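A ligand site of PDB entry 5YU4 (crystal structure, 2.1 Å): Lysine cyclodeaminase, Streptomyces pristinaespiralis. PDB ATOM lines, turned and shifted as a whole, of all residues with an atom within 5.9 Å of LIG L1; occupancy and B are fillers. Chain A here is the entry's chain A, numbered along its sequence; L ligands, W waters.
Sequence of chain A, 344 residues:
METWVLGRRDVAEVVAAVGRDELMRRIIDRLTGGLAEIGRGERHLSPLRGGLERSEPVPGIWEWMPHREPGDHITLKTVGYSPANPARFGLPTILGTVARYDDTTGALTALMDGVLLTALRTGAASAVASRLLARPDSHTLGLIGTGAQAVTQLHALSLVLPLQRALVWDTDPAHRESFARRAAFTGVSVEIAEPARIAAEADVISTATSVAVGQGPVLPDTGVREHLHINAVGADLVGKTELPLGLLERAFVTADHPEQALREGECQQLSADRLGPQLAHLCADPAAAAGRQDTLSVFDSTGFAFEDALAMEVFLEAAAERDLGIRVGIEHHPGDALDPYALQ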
ATOM      1  N   ARG A  49     -28.800  24.235  18.378  1.00  0.00           N
ATOM      2  CA  ARG A  49     -29.618  25.337  17.922  1.00  0.00           C
ATOM      3  C   ARG A  49     -31.093  25.005  18.087  1.00  0.00           C
ATOM      4  O   ARG A  49     -31.474  23.875  18.400  1.00  0.00           O
ATOM      5  CB  ARG A  49     -29.313  25.665  16.455  1.00  0.00           C
ATOM      6  CG  ARG A  49     -29.593  24.530  15.524  1.00  0.00           C
ATOM      7  CD  ARG A  49     -29.552  24.964  14.080  1.00  0.00           C
ATOM      8  NE  ARG A  49     -29.578  23.800  13.197  1.00  0.00           N
ATOM      9  CZ  ARG A  49     -28.551  23.428  12.432  1.00  0.00           C
ATOM     10  NH1 ARG A  49     -27.448  24.151  12.426  1.00  0.00           N
ATOM     11  NH2 ARG A  49     -28.641  22.358  11.648  1.00  0.00           N
ATOM     12  N   ILE A  61     -37.815  26.436   7.776  1.00  0.00           N
ATOM     13  CA  ILE A  61     -37.534  26.618   9.201  1.00  0.00           C
ATOM     14  C   ILE A  61     -36.714  27.888   9.375  1.00  0.00           C
ATOM     15  O   ILE A  61     -35.981  28.311   8.479  1.00  0.00           O
ATOM     16  CB  ILE A  61     -36.823  25.356   9.780  1.00  0.00           C
ATOM     17  CG1 ILE A  61     -36.892  25.331  11.324  1.00  0.00           C
ATOM     18  CG2 ILE A  61     -35.398  25.223   9.251  1.00  0.00           C
ATOM     19  CD1 ILE A  61     -36.343  24.024  11.934  1.00  0.00           C
ATOM     20  N   GLU A  63     -34.094  29.590  12.323  1.00  0.00           N
ATOM     21  CA  GLU A  63     -33.310  29.083  13.437  1.00  0.00           C
ATOM     22  C   GLU A  63     -32.415  30.144  14.062  1.00  0.00           C
ATOM     23  O   GLU A  63     -32.022  31.115  13.411  1.00  0.00           O
ATOM     24  CB  GLU A  63     -32.440  27.894  12.983  1.00  0.00           C
ATOM     25  CG  GLU A  63     -33.245  26.702  12.486  1.00  0.00           C
ATOM     26  CD  GLU A  63     -32.358  25.620  11.860  1.00  0.00           C
ATOM     27  OE1 GLU A  63     -31.380  25.966  11.165  1.00  0.00           O
ATOM     28  OE2 GLU A  63     -32.631  24.425  12.089  1.00  0.00           O
ATOM     29  N   MET A  65     -28.838  30.411  16.542  1.00  0.00           N
ATOM     30  CA  MET A  65     -27.638  29.624  16.778  1.00  0.00           C
ATOM     31  C   MET A  65     -26.651  30.454  17.599  1.00  0.00           C
ATOM     32  O   MET A  65     -25.921  31.288  17.027  1.00  0.00           O
ATOM     33  CB  MET A  65     -27.005  29.167  15.463  1.00  0.00           C
ATOM     34  CG  MET A  65     -28.004  28.568  14.482  1.00  0.00           C
ATOM     35  SD  MET A  65     -27.398  28.210  12.811  1.00  0.00           S
ATOM     36  CE  MET A  65     -25.858  27.339  13.149  1.00  0.00           C
ATOM     37  N   LYS A  77     -26.249  33.723  15.403  1.00  0.00           N
ATOM     38  CA  LYS A  77     -26.708  33.721  14.023  1.00  0.00           C
ATOM     39  C   LYS A  77     -28.191  33.385  13.991  1.00  0.00           C
ATOM     40  O   LYS A  77     -28.635  32.416  14.615  1.00  0.00           O
ATOM     41  CB  LYS A  77     -25.943  32.746  13.132  1.00  0.00           C
ATOM     42  CG  LYS A  77     -26.385  32.881  11.669  1.00  0.00           C
ATOM     43  CD  LYS A  77     -25.390  32.257  10.691  1.00  0.00           C
ATOM     44  CE  LYS A  77     -25.847  30.878  10.240  1.00  0.00           C
ATOM     45  NZ  LYS A  77     -24.835  30.278   9.329  1.00  0.00           N
ATOM     46  N   VAL A  79     -31.075  32.641  11.093  1.00  0.00           N
ATOM     47  CA  VAL A  79     -30.995  32.217   9.710  1.00  0.00           C
ATOM     48  C   VAL A  79     -32.262  31.459   9.327  1.00  0.00           C
ATOM     49  O   VAL A  79     -32.733  30.582  10.067  1.00  0.00           O
ATOM     50  CB  VAL A  79     -29.729  31.369   9.475  1.00  0.00           C
ATOM     51  CG1 VAL A  79     -29.681  30.207  10.452  1.00  0.00           C
ATOM     52  CG2 VAL A  79     -29.673  30.889   8.028  1.00  0.00           C
ATOM     53  N   GLY A  80     -32.801  31.783   8.153  1.00  0.00           N
ATOM     54  CA  GLY A  80     -33.980  31.138   7.636  1.00  0.00           C
ATOM     55  C   GLY A  80     -33.640  30.197   6.493  1.00  0.00           C
ATOM     56  O   GLY A  80     -32.713  30.447   5.717  1.00  0.00           O
ATOM     57  N   TYR A  81     -34.373  29.092   6.424  1.00  0.00           N
ATOM     58  CA  TYR A  81     -34.350  28.174   5.288  1.00  0.00           C
ATOM     59  C   TYR A  81     -35.727  28.257   4.669  1.00  0.00           C
ATOM     60  O   TYR A  81     -36.721  27.882   5.316  1.00  0.00           O
ATOM     61  CB  TYR A  81     -34.002  26.752   5.730  1.00  0.00           C
ATOM     62  CG  TYR A  81     -34.347  25.674   4.724  1.00  0.00           C
ATOM     63  CD1 TYR A  81     -33.536  25.434   3.624  1.00  0.00           C
ATOM     64  CD2 TYR A  81     -35.470  24.858   4.905  1.00  0.00           C
ATOM     65  CE1 TYR A  81     -33.843  24.413   2.691  1.00  0.00           C
ATOM     66  CE2 TYR A  81     -35.769  23.838   4.002  1.00  0.00           C
ATOM     67  CZ  TYR A  81     -34.958  23.625   2.888  1.00  0.00           C
ATOM     68  OH  TYR A  81     -35.264  22.608   1.997  1.00  0.00           O
ATOM     69  N   ILE A  94     -31.347  30.507   1.777  1.00  0.00           N
ATOM     70  CA  ILE A  94     -30.700  30.731   3.064  1.00  0.00           C
ATOM     71  C   ILE A  94     -30.527  32.227   3.243  1.00  0.00           C
ATOM     72  O   ILE A  94     -29.780  32.878   2.492  1.00  0.00           O
ATOM     73  CB  ILE A  94     -29.350  30.010   3.142  1.00  0.00           C
ATOM     74  CG1 ILE A  94     -29.546  28.496   3.135  1.00  0.00           C
ATOM     75  CG2 ILE A  94     -28.566  30.484   4.365  1.00  0.00           C
ATOM     76  CD1 ILE A  94     -30.389  27.965   4.271  1.00  0.00           C
ATOM     77  N   THR A 118     -22.388  32.402   5.641  1.00  0.00           N
ATOM     78  CA  THR A 118     -22.859  31.018   5.756  1.00  0.00           C
ATOM     79  C   THR A 118     -22.318  30.152   4.618  1.00  0.00           C
ATOM     80  O   THR A 118     -21.808  29.052   4.847  1.00  0.00           O
ATOM     81  CB  THR A 118     -24.399  30.962   5.774  1.00  0.00           C
ATOM     82  OG1 THR A 118     -24.898  31.588   6.956  1.00  0.00           O
ATOM     83  CG2 THR A 118     -24.870  29.512   5.740  1.00  0.00           C
ATOM     84  N   ARG A 121     -18.377  29.520   5.222  1.00  0.00           N
ATOM     85  CA  ARG A 121     -17.955  28.566   6.244  1.00  0.00           C
ATOM     86  C   ARG A 121     -18.518  27.182   5.984  1.00  0.00           C
ATOM     87  O   ARG A 121     -17.934  26.186   6.429  1.00  0.00           O
ATOM     88  CB  ARG A 121     -18.311  29.053   7.661  1.00  0.00           C
ATOM     89  CG  ARG A 121     -19.802  29.368   7.970  1.00  0.00           C
ATOM     90  CD  ARG A 121     -20.624  28.098   8.177  1.00  0.00           C
ATOM     91  NE  ARG A 121     -21.713  28.216   9.154  1.00  0.00           N
ATOM     92  CZ  ARG A 121     -22.728  27.365   9.215  1.00  0.00           C
ATOM     93  NH1 ARG A 121     -22.808  26.343   8.339  1.00  0.00           N
ATOM     94  NH2 ARG A 121     -23.665  27.516  10.139  1.00  0.00           N
ATOM     95  N   THR A 122     -19.622  27.086   5.252  1.00  0.00           N
ATOM     96  CA  THR A 122     -20.166  25.775   4.926  1.00  0.00           C
ATOM     97  C   THR A 122     -19.314  25.076   3.879  1.00  0.00           C
ATOM     98  O   THR A 122     -19.010  23.888   4.008  1.00  0.00           O
ATOM     99  CB  THR A 122     -21.614  25.923   4.461  1.00  0.00           C
ATOM    100  OG1 THR A 122     -22.376  26.515   5.508  1.00  0.00           O
ATOM    101  CG2 THR A 122     -22.223  24.550   4.114  1.00  0.00           C
ATOM    102  N   ALA A 235     -29.518  20.111   5.188  1.00  0.00           N
ATOM    103  CA  ALA A 235     -29.909  20.091   6.601  1.00  0.00           C
ATOM    104  C   ALA A 235     -30.841  21.255   6.889  1.00  0.00           C
ATOM    105  O   ALA A 235     -30.479  22.410   6.634  1.00  0.00           O
ATOM    106  CB  ALA A 235     -28.690  20.173   7.517  1.00  0.00           C
ATOM    107  N   ASP A 236     -32.021  20.952   7.411  1.00  0.00           N
ATOM    108  CA  ASP A 236     -32.982  21.967   7.820  1.00  0.00           C
ATOM    109  C   ASP A 236     -33.982  21.385   8.810  1.00  0.00           C
ATOM    110  O   ASP A 236     -33.911  21.647  10.021  1.00  0.00           O
ATOM    111  CB  ASP A 236     -33.700  22.559   6.608  1.00  0.00           C
ATOM    112  CG  ASP A 236     -34.169  21.486   5.612  1.00  0.00           C
ATOM    113  OD1 ASP A 236     -35.153  20.765   5.898  1.00  0.00           O
ATOM    114  OD2 ASP A 236     -33.526  21.375   4.533  1.00  0.00           O
ATOM    115  N   THR A 302     -24.102  19.706   9.528  1.00  0.00           N
ATOM    116  CA  THR A 302     -25.287  20.463   9.901  1.00  0.00           C
ATOM    117  C   THR A 302     -25.014  21.934  10.118  1.00  0.00           C
ATOM    118  O   THR A 302     -25.954  22.735  10.063  1.00  0.00           O
ATOM    119  CB  THR A 302     -25.941  19.904  11.171  1.00  0.00           C
ATOM    120  OG1 THR A 302     -25.024  20.049  12.277  1.00  0.00           O
ATOM    121  CG2 THR A 302     -26.310  18.441  10.982  1.00  0.00           C
ATOM    122  N   GLY A 303     -23.755  22.313  10.371  1.00  0.00           N
ATOM    123  CA  GLY A 303     -23.394  23.688  10.663  1.00  0.00           C
ATOM    124  C   GLY A 303     -23.687  24.033  12.104  1.00  0.00           C
ATOM    125  O   GLY A 303     -24.735  23.666  12.643  1.00  0.00           O
ATOM    126  N   PHE A 304     -22.763  24.720  12.761  1.00  0.00           N
ATOM    127  CA  PHE A 304     -23.030  25.133  14.134  1.00  0.00           C
ATOM    128  C   PHE A 304     -22.364  26.478  14.378  1.00  0.00           C
ATOM    129  O   PHE A 304     -21.478  26.906  13.627  1.00  0.00           O
ATOM    130  CB  PHE A 304     -22.596  24.062  15.158  1.00  0.00           C
ATOM    131  CG  PHE A 304     -21.120  23.735  15.146  1.00  0.00           C
ATOM    132  CD1 PHE A 304     -20.571  22.933  14.146  1.00  0.00           C
ATOM    133  CD2 PHE A 304     -20.298  24.161  16.181  1.00  0.00           C
ATOM    134  CE1 PHE A 304     -19.215  22.595  14.160  1.00  0.00           C
ATOM    135  CE2 PHE A 304     -18.959  23.831  16.208  1.00  0.00           C
ATOM    136  CZ  PHE A 304     -18.405  23.041  15.190  1.00  0.00           C
ATOM    137  N   GLU A 307     -18.770  27.928  13.996  1.00  0.00           N
ATOM    138  CA  GLU A 307     -18.257  28.148  12.644  1.00  0.00           C
ATOM    139  C   GLU A 307     -18.595  29.556  12.177  1.00  0.00           C
ATOM    140  O   GLU A 307     -17.771  30.230  11.551  1.00  0.00           O
ATOM    141  CB  GLU A 307     -18.838  27.121  11.666  1.00  0.00           C
ATOM    142  CG  GLU A 307     -18.546  25.654  12.029  1.00  0.00           C
ATOM    143  CD  GLU A 307     -19.216  24.664  11.087  1.00  0.00           C
ATOM    144  OE1 GLU A 307     -20.303  24.975  10.565  1.00  0.00           O
ATOM    145  OE2 GLU A 307     -18.654  23.569  10.872  1.00  0.00           O
ATOM    146  N   ASP A 308     -19.800  30.019  12.513  1.00  0.00           N
ATOM    147  CA  ASP A 308     -20.197  31.379  12.183  1.00  0.00           C
ATOM    148  C   ASP A 308     -19.387  32.407  12.949  1.00  0.00           C
ATOM    149  O   ASP A 308     -18.969  33.428  12.391  1.00  0.00           O
ATOM    150  CB  ASP A 308     -21.686  31.554  12.458  1.00  0.00           C
ATOM    151  CG  ASP A 308     -22.503  30.554  11.689  1.00  0.00           C
ATOM    152  OD1 ASP A 308     -22.467  30.616  10.444  1.00  0.00           O
ATOM    153  OD2 ASP A 308     -23.201  29.713  12.319  1.00  0.00           O
HETATM  154  N1  LIG L   1     -28.027  24.482   8.795  1.00  0.00           N
HETATM  155  C1  LIG L   1     -27.752  25.814   8.351  1.00  0.00           C
HETATM  156  C2  LIG L   1     -26.640  26.483   9.156  1.00  0.00           C
HETATM  157  O1  LIG L   1     -26.504  27.745   9.045  1.00  0.00           O
HETATM  158  C3  LIG L   1     -29.006  26.662   8.421  1.00  0.00           C
HETATM  159  C4  LIG L   1     -30.029  26.169   7.414  1.00  0.00           C
HETATM  160  N2  LIG L   1     -30.923  25.229   8.024  1.00  0.00           N
HETATM  161  O2  LIG L   1     -25.885  25.799   9.911  1.00  0.00           O
HETATM  162  P1  LG2 L   2     -30.726  26.434  -2.704  1.00  0.00           P
HETATM  163  O1  LG2 L   2     -32.215  26.562  -2.748  1.00  0.00           O
HETATM  164  O2  LG2 L   2     -29.827  27.547  -3.169  1.00  0.00           O
HETATM  165  O3  LG2 L   2     -30.310  25.116  -3.529  1.00  0.00           O
HETATM  166  C1  LG2 L   2     -30.959  23.886  -3.294  1.00  0.00           C
HETATM  167  C2  LG2 L   2     -31.018  23.157  -4.627  1.00  0.00           C
HETATM  168  O4  LG2 L   2     -31.334  21.766  -4.432  1.00  0.00           O
HETATM  169  C3  LG2 L   2     -32.086  23.738  -5.550  1.00  0.00           C
HETATM  170  O5  LG2 L   2     -31.474  24.069  -6.811  1.00  0.00           O
HETATM  171  C4  LG2 L   2     -33.088  22.600  -5.732  1.00  0.00           C
HETATM  172  O6  LG2 L   2     -33.629  22.544  -7.059  1.00  0.00           O
HETATM  173  C5  LG2 L   2     -32.212  21.391  -5.481  1.00  0.00           C
HETATM  174  N1  LG2 L   2     -32.931  20.155  -5.109  1.00  0.00           N
HETATM  175  C6  LG2 L   2     -34.068  20.029  -4.392  1.00  0.00           C
HETATM  176  N2  LG2 L   2     -34.393  18.705  -4.263  1.00  0.00           N
HETATM  177  C7  LG2 L   2     -33.454  17.994  -4.917  1.00  0.00           C
HETATM  178  C8  LG2 L   2     -33.182  16.579  -5.190  1.00  0.00           C
HETATM  179  N3  LG2 L   2     -33.996  15.605  -4.728  1.00  0.00           N
HETATM  180  N4  LG2 L   2     -32.090  16.275  -5.902  1.00  0.00           N
HETATM  181  C9  LG2 L   2     -31.245  17.209  -6.386  1.00  0.00           C
HETATM  182  N5  LG2 L   2     -31.429  18.521  -6.185  1.00  0.00           N
HETATM  183  C10 LG2 L   2     -32.499  18.954  -5.464  1.00  0.00           C
HETATM  184  O7  LG2 L   2     -30.386  26.051  -1.180  1.00  0.00           O
HETATM  185  P2  LG2 L   2     -28.918  26.076  -0.552  1.00  0.00           P
HETATM  186  O8  LG2 L   2     -27.930  25.509  -1.557  1.00  0.00           O
HETATM  187  O9  LG2 L   2     -28.693  27.431   0.053  1.00  0.00           O
HETATM  188  O10 LG2 L   2     -29.061  25.027   0.661  1.00  0.00           O
HETATM  189  C11 LG2 L   2     -29.064  23.614   0.428  1.00  0.00           C
HETATM  190  C12 LG2 L   2     -29.216  22.864   1.754  1.00  0.00           C
HETATM  191  O11 LG2 L   2     -28.058  23.079   2.561  1.00  0.00           O
HETATM  192  C13 LG2 L   2     -30.379  23.359   2.588  1.00  0.00           C
HETATM  193  O12 LG2 L   2     -30.917  22.204   3.246  1.00  0.00           O
HETATM  194  C14 LG2 L   2     -29.741  24.239   3.640  1.00  0.00           C
HETATM  195  O13 LG2 L   2     -30.567  24.356   4.795  1.00  0.00           O
HETATM  196  C15 LG2 L   2     -28.450  23.465   3.874  1.00  0.00           C
HETATM  197  N6  LG2 L   2     -27.373  24.212   4.515  1.00  0.00           N
HETATM  198  C16 LG2 L   2     -26.532  23.535   5.317  1.00  0.00           C
HETATM  199  C17 LG2 L   2     -25.474  24.175   5.954  1.00  0.00           C
HETATM  200  C18 LG2 L   2     -24.547  23.381   6.826  1.00  0.00           C
HETATM  201  O14 LG2 L   2     -23.744  23.968   7.529  1.00  0.00           O
HETATM  202  N7  LG2 L   2     -24.598  22.025   6.764  1.00  0.00           N
HETATM  203  C19 LG2 L   2     -25.285  25.551   5.763  1.00  0.00           C
HETATM  204  C20 LG2 L   2     -26.165  26.237   4.915  1.00  0.00           C
HETATM  205  C21 LG2 L   2     -27.201  25.532   4.292  1.00  0.00           C
HETATM  206  O   HOH W   1     -30.675  23.473  10.021  1.00  0.00           O
HETATM  207  O   HOH W   2     -32.234  27.574   9.030  1.00  0.00           O
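A nitrogen (N2) of LIG L1 sits close to an oxygen (O13) of LG2 L2, 3.4 Å away.
The guanidinium group (NE) of Arg 121 lies within salt-bridge range of the side-chain carboxylate (OD1) of Asp 308 (2.8 Å).
OG1 of Thr 122 sits at hydrogen-bond distance from NH1 of Arg 121, 2.9 Å away.
NH1 of Arg 121 lies within salt-bridge range of OE1 of Glu 307 (3.6 Å).
The guanidinium group (NH1) of Arg 49 lies within hydrogen-bond range of the backbone carbonyl oxygen (O) of Thr 302 (3.1 Å).
The backbone carbonyl oxygen of Lys 77 lies within hydrogen-bond range of the backbone NH of Met 65, at 2.8 Å.
The side-chain hydroxyl (OG1) of Thr 118 lies within hydrogen-bond range of the side-chain amino group (NZ) of Lys 77 (2.7 Å).
O of Gly 303 sits at hydrogen-bond distance from NH1 of Arg 49, 2.8 Å away.
The side-chain hydroxyl (OH) of Tyr 81 sits close to the side-chain carboxylate (OD2) of Asp 236 (3.3 Å).
CE of Met 65 touches O2 of LIG L1, 3.6 Å away.
Ile 94 touches LIG L1 (CD1 to C4, 3.6 Å).
Asp 236 touches LIG L1.
Gly 303 touches LIG L1.
Hydrophobic or aromatic side chains within 4 Å of LIG L1: Met 65 and Ile 94.
Ten residues have an atom within 4 Å of LIG L1: Arg 49, Glu 63, Met 65, Lys 77, Ile 94, Arg 121, Ala 235, Asp 236, Thr 302 and Gly 303.
The nearest printed residue that does not touch LIG L1 is Thr 118 (4.1 Å).
Water W1 lies within hydrogen-bond range of a nitrogen (N2) of LIG L1 (2.7 Å), the side-chain carboxylate (OE1) of Glu 63 (2.8 Å) and the guanidinium group (NH2) of Arg 49 (2.8 Å).
Water W2 lies within hydrogen-bond range of the side-chain carboxylate of Glu 63 (2.8 Å), a nitrogen (N2) of LIG L1 (2.9 Å) and the backbone carbonyl oxygen of Val 79 (3.2 Å).
NH2 of Arg 121 lies within salt-bridge range of O2 of LIG L1 (2.8 Å).
The backbone carbonyl oxygen (O) of Thr 302 sits at hydrogen-bond distance from a nitrogen (N1) of LIG L1 (3.0 Å).
An oxygen (O1) of LIG L1 is in salt-bridge range of the side-chain amino group of Lys 77, 3.0 Å away.
The backbone carbonyl oxygen of Ala 235 sits at hydrogen-bond distance from a nitrogen (N2) of LIG L1, 3.2 Å away.
A nitrogen (N2) of LIG L1 lies within salt-bridge range of the side-chain carboxylate (OE1) of Glu 63, at 3.3 Å.
The guanidinium group of Arg 49 lies within salt-bridge range of an oxygen (O2) of LIG L1, at 3.4 Å.
O14 of LG2 L2 lies within hydrogen-bond range of NH1 of Arg 121 (2.7 Å).
The backbone NH (N) of Ala 235 sits at hydrogen-bond distance from an oxygen (O12) of LG2 L2, at 3.2 Å.
An oxygen (O13) of LG2 L2 sits at hydrogen-bond distance from the backbone carbonyl oxygen (O) of Ala 235, 2.7 Å away.
N of Gly 303 sits close to O14 of LG2 L2 (3.3 Å).
OD2 of Asp 236 lies within hydrogen-bond range of O12 of LG2 L2 (3.0 Å).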
